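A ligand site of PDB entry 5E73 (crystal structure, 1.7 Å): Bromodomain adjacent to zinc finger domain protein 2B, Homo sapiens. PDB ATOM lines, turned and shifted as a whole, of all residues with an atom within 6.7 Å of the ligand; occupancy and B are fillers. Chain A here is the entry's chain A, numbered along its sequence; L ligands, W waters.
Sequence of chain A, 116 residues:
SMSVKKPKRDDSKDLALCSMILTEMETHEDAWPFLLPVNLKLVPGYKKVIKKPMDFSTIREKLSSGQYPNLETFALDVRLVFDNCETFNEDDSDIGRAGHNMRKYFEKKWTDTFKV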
ATOM      1  N   ALA A  31     -15.050 -18.887 -16.205  1.00  0.00           N
ATOM      2  CA  ALA A  31     -16.356 -18.753 -16.856  1.00  0.00           C
ATOM      3  C   ALA A  31     -17.198 -20.028 -16.744  1.00  0.00           C
ATOM      4  O   ALA A  31     -18.411 -19.989 -17.002  1.00  0.00           O
ATOM      5  CB  ALA A  31     -16.177 -18.373 -18.325  1.00  0.00           C
ATOM      6  N   TRP A  32     -16.575 -21.147 -16.367  1.00  0.00           N
ATOM      7  CA  TRP A  32     -17.228 -22.465 -16.443  1.00  0.00           C
ATOM      8  C   TRP A  32     -18.618 -22.569 -15.766  1.00  0.00           C
ATOM      9  O   TRP A  32     -19.478 -23.265 -16.306  1.00  0.00           O
ATOM     10  CB  TRP A  32     -16.307 -23.580 -15.886  1.00  0.00           C
ATOM     11  CG  TRP A  32     -15.785 -23.394 -14.473  1.00  0.00           C
ATOM     12  CD1 TRP A  32     -14.585 -22.828 -14.101  1.00  0.00           C
ATOM     13  CD2 TRP A  32     -16.421 -23.813 -13.257  1.00  0.00           C
ATOM     14  NE1 TRP A  32     -14.461 -22.854 -12.723  1.00  0.00           N
ATOM     15  CE2 TRP A  32     -15.574 -23.443 -12.195  1.00  0.00           C
ATOM     16  CE3 TRP A  32     -17.630 -24.446 -12.976  1.00  0.00           C
ATOM     17  CZ2 TRP A  32     -15.905 -23.692 -10.860  1.00  0.00           C
ATOM     18  CZ3 TRP A  32     -17.965 -24.686 -11.639  1.00  0.00           C
ATOM     19  CH2 TRP A  32     -17.105 -24.315 -10.607  1.00  0.00           C
ATOM     20  N   PRO A  33     -18.854 -21.881 -14.626  1.00  0.00           N
ATOM     21  CA  PRO A  33     -20.211 -22.046 -14.077  1.00  0.00           C
ATOM     22  C   PRO A  33     -21.311 -21.383 -14.904  1.00  0.00           C
ATOM     23  O   PRO A  33     -22.497 -21.642 -14.648  1.00  0.00           O
ATOM     24  CB  PRO A  33     -20.136 -21.359 -12.708  1.00  0.00           C
ATOM     25  CG  PRO A  33     -18.635 -21.196 -12.411  1.00  0.00           C
ATOM     26  CD  PRO A  33     -18.028 -21.011 -13.767  1.00  0.00           C
ATOM     27  N   PHE A  34     -20.915 -20.532 -15.846  1.00  0.00           N
ATOM     28  CA  PHE A  34     -21.828 -19.628 -16.530  1.00  0.00           C
ATOM     29  C   PHE A  34     -21.956 -19.918 -18.027  1.00  0.00           C
ATOM     30  O   PHE A  34     -22.591 -19.162 -18.744  1.00  0.00           O
ATOM     31  CB  PHE A  34     -21.360 -18.171 -16.310  1.00  0.00           C
ATOM     32  CG  PHE A  34     -21.007 -17.881 -14.869  1.00  0.00           C
ATOM     33  CD1 PHE A  34     -21.973 -17.947 -13.884  1.00  0.00           C
ATOM     34  CD2 PHE A  34     -19.690 -17.608 -14.497  1.00  0.00           C
ATOM     35  CE1 PHE A  34     -21.650 -17.734 -12.559  1.00  0.00           C
ATOM     36  CE2 PHE A  34     -19.364 -17.383 -13.163  1.00  0.00           C
ATOM     37  CZ  PHE A  34     -20.345 -17.453 -12.192  1.00  0.00           C
ATOM     38  N   LEU A  35     -21.341 -20.994 -18.492  1.00  0.00           N
ATOM     39  CA  LEU A  35     -21.282 -21.245 -19.934  1.00  0.00           C
ATOM     40  C   LEU A  35     -22.594 -21.822 -20.467  1.00  0.00           C
ATOM     41  O   LEU A  35     -22.907 -21.657 -21.651  1.00  0.00           O
ATOM     42  CB  LEU A  35     -20.131 -22.193 -20.272  1.00  0.00           C
ATOM     43  CG  LEU A  35     -18.757 -21.583 -20.001  1.00  0.00           C
ATOM     44  CD1 LEU A  35     -17.648 -22.563 -20.374  1.00  0.00           C
ATOM     45  CD2 LEU A  35     -18.595 -20.270 -20.759  1.00  0.00           C
ATOM     46  N   LEU A  36     -23.362 -22.477 -19.594  1.00  0.00           N
ATOM     47  CA  LEU A  36     -24.631 -23.122 -19.978  1.00  0.00           C
ATOM     48  C   LEU A  36     -25.677 -22.786 -18.923  1.00  0.00           C
ATOM     49  O   LEU A  36     -25.332 -22.412 -17.814  1.00  0.00           O
ATOM     50  CB  LEU A  36     -24.458 -24.643 -20.111  1.00  0.00           C
ATOM     51  CG  LEU A  36     -23.571 -25.166 -21.247  1.00  0.00           C
ATOM     52  CD1 LEU A  36     -23.401 -26.666 -21.154  1.00  0.00           C
ATOM     53  CD2 LEU A  36     -24.181 -24.778 -22.591  1.00  0.00           C
ATOM     54  N   PRO A  37     -26.964 -22.936 -19.251  1.00  0.00           N
ATOM     55  CA  PRO A  37     -27.966 -22.656 -18.217  1.00  0.00           C
ATOM     56  C   PRO A  37     -27.847 -23.596 -17.026  1.00  0.00           C
ATOM     57  O   PRO A  37     -27.478 -24.773 -17.189  1.00  0.00           O
ATOM     58  CB  PRO A  37     -29.290 -22.907 -18.938  1.00  0.00           C
ATOM     59  CG  PRO A  37     -28.971 -22.745 -20.407  1.00  0.00           C
ATOM     60  CD  PRO A  37     -27.562 -23.260 -20.560  1.00  0.00           C
ATOM     61  N   VAL A  38     -28.163 -23.101 -15.841  1.00  0.00           N
ATOM     62  CA  VAL A  38     -28.287 -23.968 -14.667  1.00  0.00           C
ATOM     63  C   VAL A  38     -29.362 -25.006 -14.945  1.00  0.00           C
ATOM     64  O   VAL A  38     -30.421 -24.668 -15.480  1.00  0.00           O
ATOM     65  CB  VAL A  38     -28.639 -23.163 -13.410  1.00  0.00           C
ATOM     66  CG1 VAL A  38     -28.902 -24.099 -12.215  1.00  0.00           C
ATOM     67  CG2 VAL A  38     -27.543 -22.156 -13.103  1.00  0.00           C
ATOM     68  N   ASN A  39     -29.078 -26.258 -14.613  1.00  0.00           N
ATOM     69  CA  ASN A  39     -30.041 -27.322 -14.872  1.00  0.00           C
ATOM     70  C   ASN A  39     -31.180 -27.276 -13.857  1.00  0.00           C
ATOM     71  O   ASN A  39     -31.024 -27.683 -12.698  1.00  0.00           O
ATOM     72  CB  ASN A  39     -29.355 -28.694 -14.858  1.00  0.00           C
ATOM     73  CG  ASN A  39     -30.252 -29.812 -15.378  1.00  0.00           C
ATOM     74  OD1 ASN A  39     -31.464 -29.816 -15.139  1.00  0.00           O
ATOM     75  ND2 ASN A  39     -29.667 -30.754 -16.087  1.00  0.00           N
ATOM     76  N   LEU A  40     -32.334 -26.784 -14.307  1.00  0.00           N
ATOM     77  CA  LEU A  40     -33.465 -26.548 -13.408  1.00  0.00           C
ATOM     78  C   LEU A  40     -34.058 -27.824 -12.858  1.00  0.00           C
ATOM     79  O   LEU A  40     -34.745 -27.821 -11.839  1.00  0.00           O
ATOM     80  CB  LEU A  40     -34.550 -25.735 -14.135  1.00  0.00           C
ATOM     81  CG  LEU A  40     -34.122 -24.361 -14.628  1.00  0.00           C
ATOM     82  CD1 LEU A  40     -35.326 -23.627 -15.187  1.00  0.00           C
ATOM     83  CD2 LEU A  40     -33.445 -23.540 -13.529  1.00  0.00           C
ATOM     84  N   LEU A  42     -32.141 -30.605 -12.123  1.00  0.00           N
ATOM     85  CA  LEU A  42     -31.186 -31.279 -11.252  1.00  0.00           C
ATOM     86  C   LEU A  42     -30.704 -30.417 -10.079  1.00  0.00           C
ATOM     87  O   LEU A  42     -30.030 -30.920  -9.191  1.00  0.00           O
ATOM     88  CB  LEU A  42     -29.972 -31.750 -12.066  1.00  0.00           C
ATOM     89  CG  LEU A  42     -30.265 -32.769 -13.170  1.00  0.00           C
ATOM     90  CD1 LEU A  42     -28.973 -33.184 -13.841  1.00  0.00           C
ATOM     91  CD2 LEU A  42     -31.002 -33.991 -12.624  1.00  0.00           C
ATOM     92  N   VAL A  43     -31.032 -29.138 -10.078  1.00  0.00           N
ATOM     93  CA  VAL A  43     -30.592 -28.279  -8.980  1.00  0.00           C
ATOM     94  C   VAL A  43     -31.778 -27.814  -8.134  1.00  0.00           C
ATOM     95  O   VAL A  43     -32.501 -26.884  -8.520  1.00  0.00           O
ATOM     96  CB  VAL A  43     -29.806 -27.057  -9.489  1.00  0.00           C
ATOM     97  CG1 VAL A  43     -29.305 -26.243  -8.312  1.00  0.00           C
ATOM     98  CG2 VAL A  43     -28.643 -27.504 -10.359  1.00  0.00           C
ATOM     99  N   TYR A  46     -33.423 -23.907  -7.401  1.00  0.00           N
ATOM    100  CA  TYR A  46     -33.027 -22.888  -8.369  1.00  0.00           C
ATOM    101  C   TYR A  46     -34.206 -22.308  -9.148  1.00  0.00           C
ATOM    102  O   TYR A  46     -34.342 -21.086  -9.258  1.00  0.00           O
ATOM    103  CB  TYR A  46     -31.987 -23.426  -9.352  1.00  0.00           C
ATOM    104  CG  TYR A  46     -31.171 -22.289  -9.921  1.00  0.00           C
ATOM    105  CD1 TYR A  46     -31.548 -21.639 -11.089  1.00  0.00           C
ATOM    106  CD2 TYR A  46     -30.038 -21.818  -9.252  1.00  0.00           C
ATOM    107  CE1 TYR A  46     -30.829 -20.574 -11.592  1.00  0.00           C
ATOM    108  CE2 TYR A  46     -29.295 -20.756  -9.751  1.00  0.00           C
ATOM    109  CZ  TYR A  46     -29.698 -20.136 -10.928  1.00  0.00           C
ATOM    110  OH  TYR A  46     -28.992 -19.077 -11.430  1.00  0.00           O
ATOM    111  N   MET A  54     -30.110 -16.701 -16.239  1.00  0.00           N
ATOM    112  CA  MET A  54     -29.356 -16.204 -17.393  1.00  0.00           C
ATOM    113  C   MET A  54     -27.955 -16.809 -17.379  1.00  0.00           C
ATOM    114  O   MET A  54     -27.428 -17.163 -16.314  1.00  0.00           O
ATOM    115  CB  MET A  54     -29.298 -14.667 -17.386  1.00  0.00           C
ATOM    116  CG  MET A  54     -28.673 -14.037 -18.641  1.00  0.00           C
ATOM    117  SD  MET A  54     -29.451 -14.592 -20.179  1.00  0.00           S
ATOM    118  CE  MET A  54     -31.178 -14.196 -19.883  1.00  0.00           C
ATOM    119  N   ASP A  55     -27.373 -16.973 -18.560  1.00  0.00           N
ATOM    120  CA  ASP A  55     -26.018 -17.538 -18.671  1.00  0.00           C
ATOM    121  C   ASP A  55     -25.401 -17.045 -19.961  1.00  0.00           C
ATOM    122  O   ASP A  55     -26.103 -16.485 -20.815  1.00  0.00           O
ATOM    123  CB  ASP A  55     -26.069 -19.068 -18.643  1.00  0.00           C
ATOM    124  CG  ASP A  55     -26.566 -19.645 -19.958  1.00  0.00           C
ATOM    125  OD1 ASP A  55     -27.792 -19.592 -20.206  1.00  0.00           O
ATOM    126  OD2 ASP A  55     -25.725 -20.150 -20.725  1.00  0.00           O
ATOM    127  N   VAL A  81     -26.580 -12.550 -14.703  1.00  0.00           N
ATOM    128  CA  VAL A  81     -25.817 -13.774 -14.459  1.00  0.00           C
ATOM    129  C   VAL A  81     -25.145 -13.740 -13.088  1.00  0.00           C
ATOM    130  O   VAL A  81     -25.243 -14.694 -12.305  1.00  0.00           O
ATOM    131  CB  VAL A  81     -24.744 -13.988 -15.528  1.00  0.00           C
ATOM    132  CG1 VAL A  81     -23.897 -15.259 -15.215  1.00  0.00           C
ATOM    133  CG2 VAL A  81     -25.401 -14.116 -16.894  1.00  0.00           C
ATOM    134  N   ASN A  84     -27.686 -13.427 -10.035  1.00  0.00           N
ATOM    135  CA  ASN A  84     -28.227 -14.764  -9.788  1.00  0.00           C
ATOM    136  C   ASN A  84     -27.244 -15.623  -9.028  1.00  0.00           C
ATOM    137  O   ASN A  84     -27.607 -16.308  -8.086  1.00  0.00           O
ATOM    138  CB  ASN A  84     -28.599 -15.446 -11.099  1.00  0.00           C
ATOM    139  CG  ASN A  84     -29.842 -14.875 -11.742  1.00  0.00           C
ATOM    140  OD1 ASN A  84     -30.584 -14.107 -11.120  1.00  0.00           O
ATOM    141  ND2 ASN A  84     -30.068 -15.241 -12.987  1.00  0.00           N
ATOM    142  N   CYS A  85     -25.984 -15.575  -9.453  1.00  0.00           N
ATOM    143  CA  CYS A  85     -24.926 -16.376  -8.836  1.00  0.00           C
ATOM    144  C   CYS A  85     -24.767 -16.016  -7.361  1.00  0.00           C
ATOM    145  O   CYS A  85     -24.618 -16.889  -6.509  1.00  0.00           O
ATOM    146  CB  CYS A  85     -23.595 -16.173  -9.578  1.00  0.00           C
ATOM    147  SG  CYS A  85     -22.206 -17.187  -8.947  1.00  0.00           S
ATOM    148  N   PHE A  88     -27.684 -17.346  -5.121  1.00  0.00           N
ATOM    149  CA  PHE A  88     -27.759 -18.784  -4.888  1.00  0.00           C
ATOM    150  C   PHE A  88     -26.502 -19.392  -4.252  1.00  0.00           C
ATOM    151  O   PHE A  88     -26.555 -20.467  -3.658  1.00  0.00           O
ATOM    152  CB  PHE A  88     -28.053 -19.489  -6.204  1.00  0.00           C
ATOM    153  CG  PHE A  88     -28.773 -20.793  -6.039  1.00  0.00           C
ATOM    154  CD1 PHE A  88     -30.140 -20.807  -5.776  1.00  0.00           C
ATOM    155  CD2 PHE A  88     -28.109 -21.997  -6.149  1.00  0.00           C
ATOM    156  CE1 PHE A  88     -30.819 -22.005  -5.622  1.00  0.00           C
ATOM    157  CE2 PHE A  88     -28.784 -23.204  -5.996  1.00  0.00           C
ATOM    158  CZ  PHE A  88     -30.141 -23.204  -5.732  1.00  0.00           C
ATOM    159  N   ASN A  89     -25.367 -18.725  -4.411  1.00  0.00           N
ATOM    160  CA  ASN A  89     -24.103 -19.328  -4.013  1.00  0.00           C
ATOM    161  C   ASN A  89     -23.422 -18.553  -2.892  1.00  0.00           C
ATOM    162  O   ASN A  89     -23.452 -17.328  -2.863  1.00  0.00           O
ATOM    163  CB  ASN A  89     -23.158 -19.413  -5.212  1.00  0.00           C
ATOM    164  CG  ASN A  89     -23.683 -20.327  -6.309  1.00  0.00           C
ATOM    165  OD1 ASN A  89     -23.522 -21.542  -6.244  1.00  0.00           O
ATOM    166  ND2 ASN A  89     -24.298 -19.744  -7.328  1.00  0.00           N
ATOM    167  N   ILE A  95     -18.088 -21.599  -7.173  1.00  0.00           N
ATOM    168  CA  ILE A  95     -18.984 -20.886  -8.074  1.00  0.00           C
ATOM    169  C   ILE A  95     -19.185 -19.452  -7.612  1.00  0.00           C
ATOM    170  O   ILE A  95     -19.164 -18.521  -8.425  1.00  0.00           O
ATOM    171  CB  ILE A  95     -20.340 -21.615  -8.200  1.00  0.00           C
ATOM    172  CG1 ILE A  95     -20.129 -22.971  -8.875  1.00  0.00           C
ATOM    173  CG2 ILE A  95     -21.349 -20.752  -8.979  1.00  0.00           C
ATOM    174  CD1 ILE A  95     -21.414 -23.745  -9.132  1.00  0.00           C
HETATM  175  C1  LIG L   1     -24.228 -20.557 -12.038  1.00  0.00           C
HETATM  176  C2  LIG L   1     -24.639 -21.495 -10.905  1.00  0.00           C
HETATM  177  O1  LIG L   1     -24.942 -21.030  -9.820  1.00  0.00           O
HETATM  178  N1  LIG L   1     -24.683 -22.913 -11.155  1.00  0.00           N
HETATM  179  C3  LIG L   1     -24.389 -23.484 -12.328  1.00  0.00           C
HETATM  180  C4  LIG L   1     -24.564 -24.857 -12.181  1.00  0.00           C
HETATM  181  N2  LIG L   1     -24.363 -25.856 -13.190  1.00  0.00           N
HETATM  182  C5  LIG L   1     -25.461 -26.686 -13.629  1.00  0.00           C
HETATM  183  C6  LIG L   1     -25.270 -27.730 -14.708  1.00  0.00           C
HETATM  184  O2  LIG L   1     -26.562 -26.547 -13.123  1.00  0.00           O
HETATM  185  C7  LIG L   1     -23.048 -25.973 -13.777  1.00  0.00           C
HETATM  186  C8  LIG L   1     -22.827 -25.400 -15.035  1.00  0.00           C
HETATM  187  C9  LIG L   1     -23.930 -24.678 -15.780  1.00  0.00           C
HETATM  188  C10 LIG L   1     -21.545 -25.509 -15.616  1.00  0.00           C
HETATM  189  C11 LIG L   1     -20.525 -26.165 -14.930  1.00  0.00           C
HETATM  190  C12 LIG L   1     -20.761 -26.721 -13.674  1.00  0.00           C
HETATM  191  C13 LIG L   1     -22.028 -26.629 -13.090  1.00  0.00           C
HETATM  192  O3  LIG L   1     -19.720 -27.389 -12.992  1.00  0.00           O
HETATM  193  C14 LIG L   1     -24.962 -25.105 -10.817  1.00  0.00           C
HETATM  194  C15 LIG L   1     -25.035 -23.856 -10.210  1.00  0.00           C
HETATM  195  C16 LIG L   1     -25.414 -23.748  -8.845  1.00  0.00           C
HETATM  196  C17 LIG L   1     -25.727 -24.897  -8.108  1.00  0.00           C
HETATM  197  C18 LIG L   1     -25.655 -26.166  -8.725  1.00  0.00           C
HETATM  198  C19 LIG L   1     -25.279 -26.279 -10.069  1.00  0.00           C
HETATM  199  O   HOH W   1     -26.615 -18.675 -10.453  1.00  0.00           O
HETATM  200  O   HOH W   2     -26.653 -29.605 -12.497  1.00  0.00           O
HETATM  201  O   HOH W   3     -25.494 -17.432 -12.461  1.00  0.00           O
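Merely in contact with the ligand: Trp 32 (3.1 Å), Pro 33 (3.3 Å), Phe 34 (3.9 Å), Leu 36 (3.4 Å), Pro 37 (3.8 Å), Val 38 (3.5 Å), Val 43 (3.6 Å) and Ile 95 (3.7 Å).
Ten residues have an atom within 4 Å of the ligand: Trp 32, Pro 33, Phe 34, Leu 36, Pro 37, Val 38, Asn 39, Val 43, Asn 89 and Ile 95.
Water W1 lies within hydrogen-bond range of the side-chain hydroxyl of Tyr 46, an oxygen (O1) of the ligand, the backbone NH of Cys 85 and the backbone carbonyl oxygen of Asn 84.
The side-chain amide nitrogen (ND2) of Asn 89 lies within hydrogen-bond range of the backbone carbonyl oxygen (O) of Cys 85 (3.0 Å).
N of Leu 42 sits at hydrogen-bond distance from OD1 of Asn 39.
The backbone carbonyl oxygen of Ile 95 sits at hydrogen-bond distance from the side-chain sulfur of Cys 85 (3.4 Å).
The side-chain amide nitrogen (ND2) of Asn 89 is in hydrogen-bond range of an oxygen (O1) of the ligand (2.9 Å).
N of Asn 39 sits at hydrogen-bond distance from O2 of the ligand.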
